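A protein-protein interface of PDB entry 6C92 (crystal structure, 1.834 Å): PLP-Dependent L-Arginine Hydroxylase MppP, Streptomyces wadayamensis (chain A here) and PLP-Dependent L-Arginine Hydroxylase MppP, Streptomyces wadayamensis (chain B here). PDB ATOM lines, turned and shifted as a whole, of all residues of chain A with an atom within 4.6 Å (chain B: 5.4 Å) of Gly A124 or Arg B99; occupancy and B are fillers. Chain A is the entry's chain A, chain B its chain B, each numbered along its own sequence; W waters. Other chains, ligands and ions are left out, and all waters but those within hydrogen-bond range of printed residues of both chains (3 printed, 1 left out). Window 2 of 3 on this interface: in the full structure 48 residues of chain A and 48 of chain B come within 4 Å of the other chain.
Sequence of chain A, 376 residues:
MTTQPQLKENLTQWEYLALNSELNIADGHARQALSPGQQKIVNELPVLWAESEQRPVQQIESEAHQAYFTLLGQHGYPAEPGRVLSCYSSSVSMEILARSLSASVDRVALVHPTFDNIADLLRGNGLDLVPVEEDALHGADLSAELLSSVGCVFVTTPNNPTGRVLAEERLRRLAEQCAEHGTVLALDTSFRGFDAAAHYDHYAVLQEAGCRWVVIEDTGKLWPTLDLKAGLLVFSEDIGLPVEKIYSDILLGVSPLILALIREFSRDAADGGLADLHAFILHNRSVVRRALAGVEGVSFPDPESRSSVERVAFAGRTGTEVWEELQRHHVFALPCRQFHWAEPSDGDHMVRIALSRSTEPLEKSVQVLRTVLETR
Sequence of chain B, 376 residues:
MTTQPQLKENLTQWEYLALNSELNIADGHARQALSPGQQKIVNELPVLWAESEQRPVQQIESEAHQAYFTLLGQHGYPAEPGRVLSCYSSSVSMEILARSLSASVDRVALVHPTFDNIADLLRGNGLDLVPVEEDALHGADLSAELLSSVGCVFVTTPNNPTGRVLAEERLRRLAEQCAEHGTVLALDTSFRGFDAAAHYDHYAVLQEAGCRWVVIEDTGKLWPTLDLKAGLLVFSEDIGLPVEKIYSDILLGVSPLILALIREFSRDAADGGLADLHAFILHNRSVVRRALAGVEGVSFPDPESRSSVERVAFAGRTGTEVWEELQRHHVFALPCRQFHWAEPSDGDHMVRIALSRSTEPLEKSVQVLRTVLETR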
ATOM      1  N   GLU A  95       9.580  -0.113   8.379  1.00  0.00           N
ATOM      2  CA  GLU A  95      10.113  -1.470   8.345  1.00  0.00           C
ATOM      3  C   GLU A  95       8.973  -2.484   8.390  1.00  0.00           C
ATOM      4  O   GLU A  95       8.990  -3.493   7.671  1.00  0.00           O
ATOM      5  CB  GLU A  95      11.085  -1.659   9.511  1.00  0.00           C
ATOM      6  CG  GLU A  95      11.620  -3.076   9.731  1.00  0.00           C
ATOM      7  CD  GLU A  95      12.626  -3.510   8.674  1.00  0.00           C
ATOM      8  OE1 GLU A  95      12.889  -2.716   7.751  1.00  0.00           O
ATOM      9  OE2 GLU A  95      13.184  -4.641   8.790  1.00  0.00           O
ATOM     10  N   ASP A 120      15.599   2.681   0.979  1.00  0.00           N
ATOM     11  CA  ASP A 120      16.518   1.647   1.469  1.00  0.00           C
ATOM     12  C   ASP A 120      15.799   0.584   2.300  1.00  0.00           C
ATOM     13  O   ASP A 120      16.182  -0.594   2.261  1.00  0.00           O
ATOM     14  CB  ASP A 120      17.646   2.298   2.269  1.00  0.00           C
ATOM     15  CG  ASP A 120      18.602   3.073   1.383  1.00  0.00           C
ATOM     16  OD1 ASP A 120      18.580   2.842   0.153  1.00  0.00           O
ATOM     17  OD2 ASP A 120      19.351   3.903   1.911  1.00  0.00           O
ATOM     18  N   LEU A 121      14.769   0.963   3.047  1.00  0.00           N
ATOM     19  CA  LEU A 121      13.997  -0.046   3.770  1.00  0.00           C
ATOM     20  C   LEU A 121      13.180  -0.899   2.813  1.00  0.00           C
ATOM     21  O   LEU A 121      13.032  -2.106   3.014  1.00  0.00           O
ATOM     22  CB  LEU A 121      13.094   0.614   4.808  1.00  0.00           C
ATOM     23  CG  LEU A 121      13.811   1.243   5.990  1.00  0.00           C
ATOM     24  CD1 LEU A 121      12.843   1.979   6.873  1.00  0.00           C
ATOM     25  CD2 LEU A 121      14.533   0.206   6.829  1.00  0.00           C
ATOM     26  N   LEU A 122      12.642  -0.304   1.758  1.00  0.00           N
ATOM     27  CA  LEU A 122      11.906  -1.110   0.795  1.00  0.00           C
ATOM     28  C   LEU A 122      12.841  -2.062   0.048  1.00  0.00           C
ATOM     29  O   LEU A 122      12.572  -3.270  -0.050  1.00  0.00           O
ATOM     30  CB  LEU A 122      11.153  -0.201  -0.189  1.00  0.00           C
ATOM     31  CG  LEU A 122       9.942   0.499   0.398  1.00  0.00           C
ATOM     32  CD1 LEU A 122       9.490   1.667  -0.510  1.00  0.00           C
ATOM     33  CD2 LEU A 122       8.778  -0.495   0.676  1.00  0.00           C
ATOM     34  N   ARG A 123      13.958  -1.535  -0.474  1.00  0.00           N
ATOM     35  CA  ARG A 123      14.902  -2.381  -1.201  1.00  0.00           C
ATOM     36  C   ARG A 123      15.487  -3.446  -0.302  1.00  0.00           C
ATOM     37  O   ARG A 123      15.702  -4.586  -0.733  1.00  0.00           O
ATOM     38  CB  ARG A 123      16.055  -1.556  -1.776  1.00  0.00           C
ATOM     39  CG  ARG A 123      15.674  -0.736  -2.977  1.00  0.00           C
ATOM     40  CD  ARG A 123      16.887  -0.591  -3.879  1.00  0.00           C
ATOM     41  NE  ARG A 123      16.954   0.711  -4.519  1.00  0.00           N
ATOM     42  CZ  ARG A 123      17.404   1.805  -3.914  1.00  0.00           C
ATOM     43  NH1 ARG A 123      17.805   1.755  -2.648  1.00  0.00           N
ATOM     44  NH2 ARG A 123      17.446   2.952  -4.575  1.00  0.00           N
ATOM     45  N   GLY A 124      15.790  -3.081   0.937  1.00  0.00           N
ATOM     46  CA  GLY A 124      16.361  -4.026   1.884  1.00  0.00           C
ATOM     47  C   GLY A 124      15.451  -5.201   2.180  1.00  0.00           C
ATOM     48  O   GLY A 124      15.933  -6.265   2.563  1.00  0.00           O
ATOM     49  N   ASN A 125      14.147  -5.027   2.011  1.00  0.00           N
ATOM     50  CA  ASN A 125      13.163  -6.080   2.199  1.00  0.00           C
ATOM     51  C   ASN A 125      12.736  -6.727   0.890  1.00  0.00           C
ATOM     52  O   ASN A 125      11.725  -7.421   0.854  1.00  0.00           O
ATOM     53  CB  ASN A 125      11.961  -5.501   2.936  1.00  0.00           C
ATOM     54  CG  ASN A 125      12.226  -5.381   4.418  1.00  0.00           C
ATOM     55  OD1 ASN A 125      12.230  -6.392   5.116  1.00  0.00           O
ATOM     56  ND2 ASN A 125      12.515  -4.177   4.895  1.00  0.00           N
ATOM     57  N   GLY A 126      13.464  -6.499  -0.187  1.00  0.00           N
ATOM     58  CA  GLY A 126      13.263  -7.259  -1.403  1.00  0.00           C
ATOM     59  C   GLY A 126      12.382  -6.618  -2.439  1.00  0.00           C
ATOM     60  O   GLY A 126      12.114  -7.242  -3.465  1.00  0.00           O
ATOM     61  N   MET B  94      16.737  -7.190  17.365  1.00  0.00           N
ATOM     62  CA  MET B  94      16.552  -8.527  16.804  1.00  0.00           C
ATOM     63  C   MET B  94      16.114  -8.455  15.341  1.00  0.00           C
ATOM     64  O   MET B  94      16.572  -9.246  14.521  1.00  0.00           O
ATOM     65  CB  MET B  94      15.563  -9.300  17.667  1.00  0.00           C
ATOM     66  CG  MET B  94      15.308 -10.698  17.213  1.00  0.00           C
ATOM     67  SD  MET B  94      16.792 -11.712  17.565  1.00  0.00           S
ATOM     68  CE  MET B  94      16.728 -12.827  16.166  1.00  0.00           C
ATOM     69  N   GLU B  95      15.261  -7.498  14.991  1.00  0.00           N
ATOM     70  CA  GLU B  95      14.896  -7.286  13.589  1.00  0.00           C
ATOM     71  C   GLU B  95      16.127  -6.944  12.763  1.00  0.00           C
ATOM     72  O   GLU B  95      16.306  -7.469  11.661  1.00  0.00           O
ATOM     73  CB  GLU B  95      13.857  -6.175  13.468  1.00  0.00           C
ATOM     74  CG  GLU B  95      13.501  -5.751  12.025  1.00  0.00           C
ATOM     75  CD  GLU B  95      12.664  -6.783  11.271  1.00  0.00           C
ATOM     76  OE1 GLU B  95      12.405  -7.868  11.831  1.00  0.00           O
ATOM     77  OE2 GLU B  95      12.284  -6.516  10.099  1.00  0.00           O
ATOM     78  N   ILE B  96      16.978  -6.050  13.274  1.00  0.00           N
ATOM     79  CA  ILE B  96      18.203  -5.695  12.563  1.00  0.00           C
ATOM     80  C   ILE B  96      19.071  -6.935  12.370  1.00  0.00           C
ATOM     81  O   ILE B  96      19.574  -7.211  11.268  1.00  0.00           O
ATOM     82  CB  ILE B  96      18.953  -4.571  13.313  1.00  0.00           C
ATOM     83  CG1 ILE B  96      18.142  -3.278  13.261  1.00  0.00           C
ATOM     84  CG2 ILE B  96      20.364  -4.381  12.749  1.00  0.00           C
ATOM     85  CD1 ILE B  96      18.562  -2.268  14.352  1.00  0.00           C
ATOM     86  N   LEU B  97      19.251  -7.703  13.442  1.00  0.00           N
ATOM     87  CA  LEU B  97      20.075  -8.900  13.372  1.00  0.00           C
ATOM     88  C   LEU B  97      19.487  -9.897  12.387  1.00  0.00           C
ATOM     89  O   LEU B  97      20.213 -10.519  11.591  1.00  0.00           O
ATOM     90  CB  LEU B  97      20.199  -9.526  14.770  1.00  0.00           C
ATOM     91  CG  LEU B  97      20.957 -10.852  14.803  1.00  0.00           C
ATOM     92  CD1 LEU B  97      22.383 -10.663  14.269  1.00  0.00           C
ATOM     93  CD2 LEU B  97      20.999 -11.433  16.212  1.00  0.00           C
ATOM     94  N   ALA B  98      18.171 -10.105  12.455  1.00  0.00           N
ATOM     95  CA  ALA B  98      17.546 -11.091  11.599  1.00  0.00           C
ATOM     96  C   ALA B  98      17.712 -10.705  10.139  1.00  0.00           C
ATOM     97  O   ALA B  98      18.058 -11.542   9.307  1.00  0.00           O
ATOM     98  CB  ALA B  98      16.062 -11.242  11.917  1.00  0.00           C
ATOM     99  N   ARG B  99      17.362  -9.465   9.802  1.00  0.00           N
ATOM    100  CA  ARG B  99      17.503  -9.050   8.416  1.00  0.00           C
ATOM    101  C   ARG B  99      18.965  -9.105   7.984  1.00  0.00           C
ATOM    102  O   ARG B  99      19.254  -9.436   6.827  1.00  0.00           O
ATOM    103  CB  ARG B  99      16.882  -7.662   8.212  1.00  0.00           C
ATOM    104  CG  ARG B  99      16.816  -7.303   6.732  1.00  0.00           C
ATOM    105  CD  ARG B  99      15.511  -6.693   6.332  1.00  0.00           C
ATOM    106  NE  ARG B  99      15.316  -5.332   6.776  1.00  0.00           N
ATOM    107  CZ  ARG B  99      15.977  -4.283   6.316  1.00  0.00           C
ATOM    108  NH1 ARG B  99      15.645  -3.097   6.786  1.00  0.00           N
ATOM    109  NH2 ARG B  99      16.950  -4.419   5.398  1.00  0.00           N
ATOM    110  N   SER B 100      19.900  -8.787   8.893  1.00  0.00           N
ATOM    111  CA  SER B 100      21.320  -8.879   8.574  1.00  0.00           C
ATOM    112  C   SER B 100      21.761 -10.321   8.334  1.00  0.00           C
ATOM    113  O   SER B 100      22.525 -10.586   7.399  1.00  0.00           O
ATOM    114  CB  SER B 100      22.168  -8.280   9.685  1.00  0.00           C
ATOM    115  OG  SER B 100      21.889  -6.895   9.843  1.00  0.00           O
ATOM    116  N   LEU B 101      21.320 -11.250   9.184  1.00  0.00           N
ATOM    117  CA  LEU B 101      21.611 -12.674   8.984  1.00  0.00           C
ATOM    118  C   LEU B 101      21.148 -13.146   7.618  1.00  0.00           C
ATOM    119  O   LEU B 101      21.840 -13.931   6.954  1.00  0.00           O
ATOM    120  CB  LEU B 101      20.934 -13.519  10.084  1.00  0.00           C
ATOM    121  CG  LEU B 101      21.617 -13.520  11.442  1.00  0.00           C
ATOM    122  CD1 LEU B 101      20.706 -14.083  12.550  1.00  0.00           C
ATOM    123  CD2 LEU B 101      22.947 -14.317  11.358  1.00  0.00           C
ATOM    124  N   SER B 102      19.972 -12.693   7.179  1.00  0.00           N
ATOM    125  CA  SER B 102      19.411 -13.228   5.955  1.00  0.00           C
ATOM    126  C   SER B 102      20.241 -12.859   4.731  1.00  0.00           C
ATOM    127  O   SER B 102      20.031 -13.462   3.682  1.00  0.00           O
ATOM    128  CB  SER B 102      17.960 -12.766   5.760  1.00  0.00           C
ATOM    129  OG  SER B 102      17.905 -11.418   5.373  1.00  0.00           O
ATOM    130  N   ALA B 103      21.195 -11.919   4.852  1.00  0.00           N
ATOM    131  CA  ALA B 103      22.093 -11.589   3.743  1.00  0.00           C
ATOM    132  C   ALA B 103      23.031 -12.740   3.389  1.00  0.00           C
ATOM    133  O   ALA B 103      23.441 -12.854   2.233  1.00  0.00           O
ATOM    134  CB  ALA B 103      22.922 -10.347   4.084  1.00  0.00           C
ATOM    135  N   ASN B 125      12.107 -13.039   8.371  1.00  0.00           N
ATOM    136  CA  ASN B 125      13.162 -12.569   7.490  1.00  0.00           C
ATOM    137  C   ASN B 125      13.766 -13.688   6.650  1.00  0.00           C
ATOM    138  O   ASN B 125      14.831 -13.497   6.068  1.00  0.00           O
ATOM    139  CB  ASN B 125      14.240 -11.866   8.314  1.00  0.00           C
ATOM    140  CG  ASN B 125      13.834 -10.464   8.690  1.00  0.00           C
ATOM    141  OD1 ASN B 125      13.943  -9.543   7.874  1.00  0.00           O
ATOM    142  ND2 ASN B 125      13.343 -10.284   9.916  1.00  0.00           N
ATOM    143  N   ILE B 246      22.101  -1.768   8.301  1.00  0.00           N
ATOM    144  CA  ILE B 246      20.662  -1.880   8.506  1.00  0.00           C
ATOM    145  C   ILE B 246      20.230  -1.070   9.724  1.00  0.00           C
ATOM    146  O   ILE B 246      19.201  -0.382   9.687  1.00  0.00           O
ATOM    147  CB  ILE B 246      20.269  -3.367   8.588  1.00  0.00           C
ATOM    148  CG1 ILE B 246      20.467  -4.008   7.215  1.00  0.00           C
ATOM    149  CG2 ILE B 246      18.813  -3.531   9.051  1.00  0.00           C
ATOM    150  CD1 ILE B 246      20.200  -5.493   7.169  1.00  0.00           C
ATOM    151  N   ASP B 249      19.708   2.323   8.505  1.00  0.00           N
ATOM    152  CA  ASP B 249      18.471   2.482   7.747  1.00  0.00           C
ATOM    153  C   ASP B 249      17.291   2.713   8.670  1.00  0.00           C
ATOM    154  O   ASP B 249      16.348   3.415   8.293  1.00  0.00           O
ATOM    155  CB  ASP B 249      18.181   1.260   6.882  1.00  0.00           C
ATOM    156  CG  ASP B 249      19.184   1.065   5.758  1.00  0.00           C
ATOM    157  OD1 ASP B 249      19.812   2.065   5.324  1.00  0.00           O
ATOM    158  OD2 ASP B 249      19.310  -0.089   5.304  1.00  0.00           O
ATOM    159  N   ILE B 250      17.333   2.158   9.885  1.00  0.00           N
ATOM    160  CA  ILE B 250      16.182   2.251  10.792  1.00  0.00           C
ATOM    161  C   ILE B 250      16.267   3.460  11.714  1.00  0.00           C
ATOM    162  O   ILE B 250      15.246   4.101  11.968  1.00  0.00           O
ATOM    163  CB  ILE B 250      16.016   0.937  11.582  1.00  0.00           C
ATOM    164  CG1 ILE B 250      15.562  -0.189  10.626  1.00  0.00           C
ATOM    165  CG2 ILE B 250      14.966   1.074  12.702  1.00  0.00           C
ATOM    166  CD1 ILE B 250      15.627  -1.527  11.185  1.00  0.00           C
HETATM  167  O   HOH W   1      18.913   4.513   4.500  1.00  0.00           O
HETATM  168  O   HOH W   2      17.261  -1.691   4.782  1.00  0.00           O
HETATM  169  O   HOH W   3      18.413  -6.200   4.004  1.00  0.00           O
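The side-chain carboxylate of Glu A95 lies close to the side-chain carboxylate of Glu B95 (2.5 Å). The side-chain carboxylate (OE1) of Glu A95 lies within salt-bridge range of the guanidinium group (NH1) of Arg B99 (2.9 Å).
The side-chain carboxylate of Glu A95 lies within hydrogen-bond range of the side-chain amide nitrogen of Asn A125. The side-chain carboxylate (OD1) of Asp A120 is in salt-bridge range of the guanidinium group (NH1) of Arg A123 (3.1 Å). O of Leu A121 sits at hydrogen-bond distance from ND2 of Asn A125. The side-chain amide nitrogen of Asn B125 is in hydrogen-bond range of the side-chain carboxylate of Glu B95 (3.2 Å). The backbone carbonyl oxygen of Arg B99 is in hydrogen-bond range of the side-chain hydroxyl of Ser B102 (2.8 Å).
Among the printed residues, merely in contact across the chains: Asp A120 with Asp B249, Leu A121 with Arg B99, Leu A121 with Asp B249, Leu A121 with Ile B250, Gly A124 with Arg B99 and Asn A125 with Arg B99.
Gly A124 touches just one residue of chain B: Arg B99. Printed residues of chain A within 4 Å of Arg B99: Glu A95 (2.9 Å), Leu A121 (3.5 Å), Gly A124 (3.5 Å) and Asn A125 (3.5 Å). Printed residues of chain B within 4 Å of Asp A120: Asp B249 (3.8 Å). Printed residues of chain B within 4 Å of Leu A121: Arg B99, Asp B249 and Ile B250. Of the printed residues of chain A, Glu B95 touches Glu A95 (2.5 Å). The nearest printed residue of chain A that does not touch Arg B99 is Asp A120 (5.0 Å).
Of the 14 printed residues of chain B, 4 touch a printed residue of chain A. Hydrophobic or aromatic side chains of chain A within 4 Å of the printed part of chain B: Leu A121.
Water W2 lies within hydrogen-bond range of the side-chain carboxylate (OD2) of Asp B249, the guanidinium group (NH2) of Arg B99 and the backbone carbonyl oxygen (O) of Asp A120. Water W3 lies within hydrogen-bond range of the guanidinium group (NH2) of Arg B99 (2.7 Å) and the backbone carbonyl oxygen (O) of Gly A124 (2.9 Å). Water W1 bridges OD2 of Asp A120 and OD1 of Asp B249.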
